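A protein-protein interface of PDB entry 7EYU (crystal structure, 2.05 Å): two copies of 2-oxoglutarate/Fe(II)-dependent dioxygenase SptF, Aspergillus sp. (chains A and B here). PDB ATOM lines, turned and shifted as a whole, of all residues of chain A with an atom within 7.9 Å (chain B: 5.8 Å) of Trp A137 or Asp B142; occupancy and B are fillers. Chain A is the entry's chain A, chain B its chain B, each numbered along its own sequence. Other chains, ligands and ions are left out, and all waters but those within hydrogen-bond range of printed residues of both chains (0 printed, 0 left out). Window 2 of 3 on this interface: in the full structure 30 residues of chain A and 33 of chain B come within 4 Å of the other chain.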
ATOM      1  N   TYR A 132       4.391 -12.331 -19.215  1.00  0.00           N
ATOM      2  CA  TYR A 132       4.922 -13.519 -18.559  1.00  0.00           C
ATOM      3  C   TYR A 132       3.772 -14.255 -17.880  1.00  0.00           C
ATOM      4  O   TYR A 132       3.099 -13.692 -17.010  1.00  0.00           O
ATOM      5  CB  TYR A 132       5.995 -13.155 -17.534  1.00  0.00           C
ATOM      6  CG  TYR A 132       7.266 -12.586 -18.121  1.00  0.00           C
ATOM      7  CD1 TYR A 132       8.318 -13.415 -18.490  1.00  0.00           C
ATOM      8  CD2 TYR A 132       7.423 -11.219 -18.291  1.00  0.00           C
ATOM      9  CE1 TYR A 132       9.484 -12.897 -19.022  1.00  0.00           C
ATOM     10  CE2 TYR A 132       8.583 -10.692 -18.819  1.00  0.00           C
ATOM     11  CZ  TYR A 132       9.611 -11.533 -19.184  1.00  0.00           C
ATOM     12  OH  TYR A 132      10.767 -11.005 -19.713  1.00  0.00           O
ATOM     13  N   GLN A 133       3.542 -15.507 -18.282  1.00  0.00           N
ATOM     14  CA  GLN A 133       2.493 -16.293 -17.644  1.00  0.00           C
ATOM     15  C   GLN A 133       2.823 -16.585 -16.186  1.00  0.00           C
ATOM     16  O   GLN A 133       1.913 -16.688 -15.355  1.00  0.00           O
ATOM     17  CB  GLN A 133       2.268 -17.596 -18.411  1.00  0.00           C
ATOM     18  N   ILE A 134       4.113 -16.711 -15.857  1.00  0.00           N
ATOM     19  CA  ILE A 134       4.526 -16.987 -14.481  1.00  0.00           C
ATOM     20  C   ILE A 134       4.417 -15.773 -13.576  1.00  0.00           C
ATOM     21  O   ILE A 134       4.751 -15.868 -12.389  1.00  0.00           O
ATOM     22  CB  ILE A 134       5.972 -17.519 -14.439  1.00  0.00           C
ATOM     23  CG1 ILE A 134       6.915 -16.551 -15.155  1.00  0.00           C
ATOM     24  CG2 ILE A 134       6.048 -18.904 -15.065  1.00  0.00           C
ATOM     25  CD1 ILE A 134       8.303 -17.102 -15.365  1.00  0.00           C
ATOM     26  N   SER A 135       3.967 -14.628 -14.098  1.00  0.00           N
ATOM     27  CA  SER A 135       3.721 -13.474 -13.243  1.00  0.00           C
ATOM     28  C   SER A 135       2.541 -13.701 -12.310  1.00  0.00           C
ATOM     29  O   SER A 135       2.471 -13.070 -11.251  1.00  0.00           O
ATOM     30  CB  SER A 135       3.485 -12.224 -14.092  1.00  0.00           C
ATOM     31  OG  SER A 135       2.343 -12.370 -14.918  1.00  0.00           O
ATOM     32  N   LYS A 136       1.614 -14.589 -12.681  1.00  0.00           N
ATOM     33  CA  LYS A 136       0.500 -14.912 -11.797  1.00  0.00           C
ATOM     34  C   LYS A 136       0.966 -15.692 -10.575  1.00  0.00           C
ATOM     35  O   LYS A 136       0.337 -15.611  -9.513  1.00  0.00           O
ATOM     36  CB  LYS A 136      -0.565 -15.704 -12.558  1.00  0.00           C
ATOM     37  CG  LYS A 136      -1.442 -14.864 -13.478  1.00  0.00           C
ATOM     38  CD  LYS A 136      -0.794 -14.661 -14.839  1.00  0.00           C
ATOM     39  CE  LYS A 136      -1.813 -14.767 -15.961  1.00  0.00           C
ATOM     40  NZ  LYS A 136      -2.852 -13.703 -15.878  1.00  0.00           N
ATOM     41  N   TRP A 137       2.057 -16.450 -10.703  1.00  0.00           N
ATOM     42  CA  TRP A 137       2.612 -17.172  -9.565  1.00  0.00           C
ATOM     43  C   TRP A 137       3.455 -16.280  -8.667  1.00  0.00           C
ATOM     44  O   TRP A 137       3.656 -16.615  -7.493  1.00  0.00           O
ATOM     45  CB  TRP A 137       3.482 -18.343 -10.034  1.00  0.00           C
ATOM     46  CG  TRP A 137       2.871 -19.249 -11.065  1.00  0.00           C
ATOM     47  CD1 TRP A 137       1.572 -19.273 -11.483  1.00  0.00           C
ATOM     48  CD2 TRP A 137       3.549 -20.271 -11.804  1.00  0.00           C
ATOM     49  NE1 TRP A 137       1.400 -20.245 -12.440  1.00  0.00           N
ATOM     50  CE2 TRP A 137       2.600 -20.872 -12.653  1.00  0.00           C
ATOM     51  CE3 TRP A 137       4.867 -20.735 -11.830  1.00  0.00           C
ATOM     52  CZ2 TRP A 137       2.928 -21.913 -13.518  1.00  0.00           C
ATOM     53  CZ3 TRP A 137       5.192 -21.766 -12.688  1.00  0.00           C
ATOM     54  CH2 TRP A 137       4.226 -22.345 -13.519  1.00  0.00           C
ATOM     55  N   ARG A 138       3.947 -15.162  -9.190  1.00  0.00           N
ATOM     56  CA  ARG A 138       4.916 -14.341  -8.481  1.00  0.00           C
ATOM     57  C   ARG A 138       4.236 -13.460  -7.441  1.00  0.00           C
ATOM     58  O   ARG A 138       3.127 -12.960  -7.654  1.00  0.00           O
ATOM     59  CB  ARG A 138       5.692 -13.477  -9.477  1.00  0.00           C
ATOM     60  CG  ARG A 138       6.717 -12.549  -8.851  1.00  0.00           C
ATOM     61  CD  ARG A 138       7.425 -11.723  -9.910  1.00  0.00           C
ATOM     62  NE  ARG A 138       8.173 -10.616  -9.325  1.00  0.00           N
ATOM     63  CZ  ARG A 138       7.648  -9.429  -9.040  1.00  0.00           C
ATOM     64  NH1 ARG A 138       6.367  -9.193  -9.285  1.00  0.00           N
ATOM     65  NH2 ARG A 138       8.404  -8.478  -8.509  1.00  0.00           N
ATOM     66  N   ARG A 139       4.913 -13.275  -6.305  1.00  0.00           N
ATOM     67  CA  ARG A 139       4.534 -12.414  -5.200  1.00  0.00           C
ATOM     68  C   ARG A 139       5.273 -11.083  -5.293  1.00  0.00           C
ATOM     69  O   ARG A 139       6.357 -11.012  -5.881  1.00  0.00           O
ATOM     70  CB  ARG A 139       4.853 -13.098  -3.867  1.00  0.00           C
ATOM     71  CG  ARG A 139       4.168 -14.447  -3.699  1.00  0.00           C
ATOM     72  CD  ARG A 139       2.683 -14.314  -3.971  1.00  0.00           C
ATOM     73  NE  ARG A 139       2.104 -13.300  -3.098  1.00  0.00           N
ATOM     74  CZ  ARG A 139       1.452 -13.566  -1.973  1.00  0.00           C
ATOM     75  NH1 ARG A 139       1.275 -14.823  -1.588  1.00  0.00           N
ATOM     76  NH2 ARG A 139       0.973 -12.576  -1.236  1.00  0.00           N
ATOM     77  N   PRO A 140       4.712 -10.003  -4.740  1.00  0.00           N
ATOM     78  CA  PRO A 140       5.369  -8.689  -4.867  1.00  0.00           C
ATOM     79  C   PRO A 140       6.762  -8.632  -4.262  1.00  0.00           C
ATOM     80  O   PRO A 140       7.549  -7.756  -4.644  1.00  0.00           O
ATOM     81  CB  PRO A 140       4.406  -7.742  -4.136  1.00  0.00           C
ATOM     82  CG  PRO A 140       3.087  -8.434  -4.184  1.00  0.00           C
ATOM     83  CD  PRO A 140       3.395  -9.898  -4.088  1.00  0.00           C
ATOM     84  N   ASP A 142       8.993 -11.102  -4.519  1.00  0.00           N
ATOM     85  CA  ASP A 142       9.901 -11.890  -5.332  1.00  0.00           C
ATOM     86  C   ASP A 142      10.720 -10.985  -6.247  1.00  0.00           C
ATOM     87  O   ASP A 142      10.327  -9.850  -6.527  1.00  0.00           O
ATOM     88  CB  ASP A 142       9.118 -12.903  -6.161  1.00  0.00           C
ATOM     89  CG  ASP A 142       8.569 -14.042  -5.326  1.00  0.00           C
ATOM     90  OD1 ASP A 142       9.187 -14.376  -4.293  1.00  0.00           O
ATOM     91  OD2 ASP A 142       7.520 -14.606  -5.705  1.00  0.00           O
ATOM     92  N   LEU A 145      10.807 -10.105 -12.927  1.00  0.00           N
ATOM     93  CA  LEU A 145      10.946 -10.989 -14.077  1.00  0.00           C
ATOM     94  C   LEU A 145      11.719 -10.346 -15.219  1.00  0.00           C
ATOM     95  O   LEU A 145      12.214 -11.064 -16.094  1.00  0.00           O
ATOM     96  CB  LEU A 145       9.566 -11.426 -14.576  1.00  0.00           C
ATOM     97  CG  LEU A 145       8.655 -12.112 -13.558  1.00  0.00           C
ATOM     98  CD1 LEU A 145       7.258 -12.299 -14.132  1.00  0.00           C
ATOM     99  CD2 LEU A 145       9.242 -13.445 -13.121  1.00  0.00           C
ATOM    100  N   ASN A 174      -1.113  -9.252  -7.585  1.00  0.00           N
ATOM    101  CA  ASN A 174      -1.341  -9.544  -8.997  1.00  0.00           C
ATOM    102  C   ASN A 174      -2.715  -9.078  -9.464  1.00  0.00           C
ATOM    103  O   ASN A 174      -2.866  -8.650 -10.614  1.00  0.00           O
ATOM    104  CB  ASN A 174      -1.172 -11.041  -9.256  1.00  0.00           C
ATOM    105  CG  ASN A 174       0.094 -11.358 -10.025  1.00  0.00           C
ATOM    106  OD1 ASN A 174       0.441 -10.670 -10.985  1.00  0.00           O
ATOM    107  ND2 ASN A 174       0.795 -12.403  -9.602  1.00  0.00           N
ATOM    108  N   TYR B 103       0.513 -21.413 -21.797  1.00  0.00           N
ATOM    109  CA  TYR B 103       1.704 -20.766 -22.326  1.00  0.00           C
ATOM    110  C   TYR B 103       1.637 -20.505 -23.824  1.00  0.00           C
ATOM    111  O   TYR B 103       2.464 -19.745 -24.340  1.00  0.00           O
ATOM    112  CB  TYR B 103       2.938 -21.618 -22.016  1.00  0.00           C
ATOM    113  CG  TYR B 103       3.125 -21.915 -20.546  1.00  0.00           C
ATOM    114  CD1 TYR B 103       3.837 -21.048 -19.729  1.00  0.00           C
ATOM    115  CD2 TYR B 103       2.595 -23.067 -19.978  1.00  0.00           C
ATOM    116  CE1 TYR B 103       4.014 -21.316 -18.386  1.00  0.00           C
ATOM    117  CE2 TYR B 103       2.768 -23.343 -18.637  1.00  0.00           C
ATOM    118  CZ  TYR B 103       3.477 -22.466 -17.847  1.00  0.00           C
ATOM    119  OH  TYR B 103       3.647 -22.742 -16.511  1.00  0.00           O
ATOM    120  N   ILE B 134      11.780 -21.309 -10.858  1.00  0.00           N
ATOM    121  CA  ILE B 134      10.370 -20.958 -10.716  1.00  0.00           C
ATOM    122  C   ILE B 134       9.565 -22.171 -10.267  1.00  0.00           C
ATOM    123  O   ILE B 134       8.354 -22.074 -10.045  1.00  0.00           O
ATOM    124  CB  ILE B 134       9.810 -20.388 -12.030  1.00  0.00           C
ATOM    125  CG1 ILE B 134       9.756 -21.479 -13.101  1.00  0.00           C
ATOM    126  CG2 ILE B 134      10.649 -19.213 -12.502  1.00  0.00           C
ATOM    127  CD1 ILE B 134       9.270 -20.991 -14.444  1.00  0.00           C
ATOM    128  N   TRP B 137       7.847 -21.535  -7.093  1.00  0.00           N
ATOM    129  CA  TRP B 137       6.638 -20.724  -7.152  1.00  0.00           C
ATOM    130  C   TRP B 137       5.434 -21.515  -7.639  1.00  0.00           C
ATOM    131  O   TRP B 137       4.294 -21.080  -7.431  1.00  0.00           O
ATOM    132  CB  TRP B 137       6.826 -19.516  -8.077  1.00  0.00           C
ATOM    133  CG  TRP B 137       8.045 -18.676  -7.807  1.00  0.00           C
ATOM    134  CD1 TRP B 137       8.872 -18.749  -6.723  1.00  0.00           C
ATOM    135  CD2 TRP B 137       8.553 -17.616  -8.629  1.00  0.00           C
ATOM    136  NE1 TRP B 137       9.872 -17.813  -6.828  1.00  0.00           N
ATOM    137  CE2 TRP B 137       9.698 -17.103  -7.988  1.00  0.00           C
ATOM    138  CE3 TRP B 137       8.155 -17.058  -9.846  1.00  0.00           C
ATOM    139  CZ2 TRP B 137      10.446 -16.060  -8.523  1.00  0.00           C
ATOM    140  CZ3 TRP B 137       8.900 -16.022 -10.376  1.00  0.00           C
ATOM    141  CH2 TRP B 137      10.032 -15.533  -9.714  1.00  0.00           C
ATOM    142  N   ARG B 138       5.664 -22.660  -8.278  1.00  0.00           N
ATOM    143  CA  ARG B 138       4.595 -23.458  -8.854  1.00  0.00           C
ATOM    144  C   ARG B 138       3.916 -24.314  -7.790  1.00  0.00           C
ATOM    145  O   ARG B 138       4.549 -24.796  -6.846  1.00  0.00           O
ATOM    146  CB  ARG B 138       5.147 -24.346  -9.971  1.00  0.00           C
ATOM    147  CG  ARG B 138       4.105 -25.200 -10.678  1.00  0.00           C
ATOM    148  CD  ARG B 138       4.738 -26.122 -11.707  1.00  0.00           C
ATOM    149  NE  ARG B 138       3.806 -27.153 -12.158  1.00  0.00           N
ATOM    150  CZ  ARG B 138       3.631 -28.321 -11.549  1.00  0.00           C
ATOM    151  NH1 ARG B 138       4.328 -28.612 -10.459  1.00  0.00           N
ATOM    152  NH2 ARG B 138       2.760 -29.200 -12.027  1.00  0.00           N
ATOM    153  N   ARG B 139       2.610 -24.492  -7.953  1.00  0.00           N
ATOM    154  CA  ARG B 139       1.785 -25.358  -7.130  1.00  0.00           C
ATOM    155  C   ARG B 139       1.459 -26.643  -7.877  1.00  0.00           C
ATOM    156  O   ARG B 139       1.522 -26.688  -9.110  1.00  0.00           O
ATOM    157  CB  ARG B 139       0.491 -24.637  -6.734  1.00  0.00           C
ATOM    158  CG  ARG B 139       0.698 -23.500  -5.745  1.00  0.00           C
ATOM    159  CD  ARG B 139       0.754 -24.013  -4.313  1.00  0.00           C
ATOM    160  NE  ARG B 139      -0.570 -24.078  -3.700  1.00  0.00           N
ATOM    161  CZ  ARG B 139      -0.785 -24.266  -2.401  1.00  0.00           C
ATOM    162  NH1 ARG B 139       0.240 -24.409  -1.570  1.00  0.00           N
ATOM    163  NH2 ARG B 139      -2.023 -24.311  -1.931  1.00  0.00           N
ATOM    164  N   PRO B 140       1.119 -27.720  -7.162  1.00  0.00           N
ATOM    165  CA  PRO B 140       0.843 -28.994  -7.850  1.00  0.00           C
ATOM    166  C   PRO B 140      -0.302 -28.921  -8.846  1.00  0.00           C
ATOM    167  O   PRO B 140      -0.329 -29.712  -9.799  1.00  0.00           O
ATOM    168  CB  PRO B 140       0.521 -29.952  -6.694  1.00  0.00           C
ATOM    169  CG  PRO B 140       1.198 -29.357  -5.511  1.00  0.00           C
ATOM    170  CD  PRO B 140       1.115 -27.873  -5.696  1.00  0.00           C
ATOM    171  N   THR B 141      -1.249 -28.003  -8.662  1.00  0.00           N
ATOM    172  CA  THR B 141      -2.373 -27.872  -9.581  1.00  0.00           C
ATOM    173  C   THR B 141      -2.047 -27.029 -10.806  1.00  0.00           C
ATOM    174  O   THR B 141      -2.893 -26.910 -11.700  1.00  0.00           O
ATOM    175  CB  THR B 141      -3.582 -27.275  -8.855  1.00  0.00           C
ATOM    176  OG1 THR B 141      -3.162 -26.164  -8.056  1.00  0.00           O
ATOM    177  CG2 THR B 141      -4.232 -28.321  -7.960  1.00  0.00           C
ATOM    178  N   ASP B 142      -0.856 -26.444 -10.873  1.00  0.00           N
ATOM    179  CA  ASP B 142      -0.442 -25.675 -12.032  1.00  0.00           C
ATOM    180  C   ASP B 142       0.032 -26.607 -13.144  1.00  0.00           C
ATOM    181  O   ASP B 142       0.356 -27.771 -12.895  1.00  0.00           O
ATOM    182  CB  ASP B 142       0.669 -24.705 -11.645  1.00  0.00           C
ATOM    183  CG  ASP B 142       0.190 -23.611 -10.712  1.00  0.00           C
ATOM    184  OD1 ASP B 142      -0.912 -23.070 -10.945  1.00  0.00           O
ATOM    185  OD2 ASP B 142       0.915 -23.290  -9.748  1.00  0.00           O
ATOM    186  N   PRO B 143       0.066 -26.125 -14.387  1.00  0.00           N
ATOM    187  CA  PRO B 143       0.626 -26.941 -15.470  1.00  0.00           C
ATOM    188  C   PRO B 143       2.103 -27.225 -15.244  1.00  0.00           C
ATOM    189  O   PRO B 143       2.810 -26.490 -14.550  1.00  0.00           O
ATOM    190  CB  PRO B 143       0.406 -26.079 -16.721  1.00  0.00           C
ATOM    191  CG  PRO B 143       0.191 -24.691 -16.205  1.00  0.00           C
ATOM    192  CD  PRO B 143      -0.502 -24.864 -14.891  1.00  0.00           C
ATOM    193  N   ASP B 144       2.569 -28.315 -15.846  1.00  0.00           N
ATOM    194  CA  ASP B 144       3.955 -28.727 -15.682  1.00  0.00           C
ATOM    195  C   ASP B 144       4.896 -27.763 -16.398  1.00  0.00           C
ATOM    196  O   ASP B 144       4.540 -27.137 -17.399  1.00  0.00           O
ATOM    197  CB  ASP B 144       4.157 -30.146 -16.212  1.00  0.00           C
ATOM    198  CG  ASP B 144       3.771 -31.208 -15.201  1.00  0.00           C
ATOM    199  OD1 ASP B 144       4.417 -31.277 -14.133  1.00  0.00           O
ATOM    200  OD2 ASP B 144       2.820 -31.971 -15.470  1.00  0.00           O
ATOM    201  N   LEU B 145       6.114 -27.649 -15.864  1.00  0.00           N
ATOM    202  CA  LEU B 145       7.131 -26.798 -16.470  1.00  0.00           C
ATOM    203  C   LEU B 145       7.835 -27.470 -17.638  1.00  0.00           C
ATOM    204  O   LEU B 145       8.442 -26.775 -18.462  1.00  0.00           O
ATOM    205  CB  LEU B 145       8.166 -26.386 -15.421  1.00  0.00           C
ATOM    206  CG  LEU B 145       7.633 -25.667 -14.183  1.00  0.00           C
ATOM    207  CD1 LEU B 145       8.767 -25.341 -13.223  1.00  0.00           C
ATOM    208  CD2 LEU B 145       6.887 -24.406 -14.583  1.00  0.00           C
ATOM    209  N   PHE B 226      10.386 -20.328 -21.944  1.00  0.00           N
ATOM    210  CA  PHE B 226      11.485 -20.849 -21.143  1.00  0.00           C
ATOM    211  C   PHE B 226      12.683 -21.146 -22.037  1.00  0.00           C
ATOM    212  O   PHE B 226      12.527 -21.658 -23.151  1.00  0.00           O
ATOM    213  CB  PHE B 226      11.070 -22.116 -20.386  1.00  0.00           C
ATOM    214  CG  PHE B 226       9.930 -21.908 -19.428  1.00  0.00           C
ATOM    215  CD1 PHE B 226       9.649 -20.648 -18.924  1.00  0.00           C
ATOM    216  CD2 PHE B 226       9.140 -22.973 -19.029  1.00  0.00           C
ATOM    217  CE1 PHE B 226       8.601 -20.454 -18.044  1.00  0.00           C
ATOM    218  CE2 PHE B 226       8.091 -22.786 -18.149  1.00  0.00           C
ATOM    219  CZ  PHE B 226       7.822 -21.524 -17.656  1.00  0.00           C
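Of the 12 printed residues of chain A, 3 touch a printed residue of chain B.
Printed residues of chain A that touch a printed residue of chain B: Ile A134, Trp A137 and Leu A145.
Hydrophobic or aromatic side chains of chain A that line the printed part of chain B: Ile A134, Trp A137 and Leu A145.
Among the printed residues, no Asp or Glu carboxylate lies within 4 Å of a Lys or Arg side-chain nitrogen of the other chain.
Ile B134 touches its own counterpart, Ile A134.
Trp A137 touches its own counterpart, Trp B137.
Trp A137 touches Asp B142, but with the chains exchanged Asp A142 does not touch Trp B137 (4.02 Å).
Trp A137 touches Leu B145, and with the chains exchanged Leu A145 touches Trp B137.
Of chain B, only Tyr B103 (3.1 Å), Trp B137 (3.9 Å), Arg B138 (3.7 Å), Asp B142 (3.9 Å) and Leu B145 (3.5 Å) come within 4 Å of Trp A137.
Of chain A, only Trp A137 comes within 4 Å of Asp B142.
No residue of chain A comes within 4 Å of Pro B143.
Of the printed residues of chain B, Leu A145 touches Trp B137 (3.8 Å).
Of the printed residues of chain A, Arg B138 touches Trp A137 (3.7 Å).
Printed residues of chain A within 4 Å of Tyr B103: Trp A137 (3.1 Å).
Lys A136 touches none of the printed residues of chain B.
The nearest printed residue of chain A that does not touch Leu B145 is Ile A134 (5.6 Å).
CD1 of Ile B134 touches CG2 of Ile A134, 3.9 Å away.
CH2 of Trp A137 touches OH of Tyr B103, at 3.1 Å.
Trp A137 touches Trp B137.
Trp A137 touches Arg B138 (CZ3 to CB, 3.7 Å).
NE1 of Trp A137 touches OD1 of Asp B142, 3.9 Å away.
CH2 of Trp A137 touches CD2 of Leu B145 (3.5 Å).
Trp B137 touches Leu A145.
The guanidinium group of Arg B138 is in salt-bridge range of the side-chain carboxylate of Asp B144 (3.4 Å).
OD2 of Asp B142 lies within hydrogen-bond range of N of Arg B139 (2.7 Å).
The backbone carbonyl oxygen (O) of Asp B142 sits at hydrogen-bond distance from the guanidinium group (NH2) of Arg B138 (2.9 Å).
The guanidinium group (NE) of Arg B138 is in hydrogen-bond range of the backbone carbonyl oxygen (O) of Pro B143 (2.7 Å).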
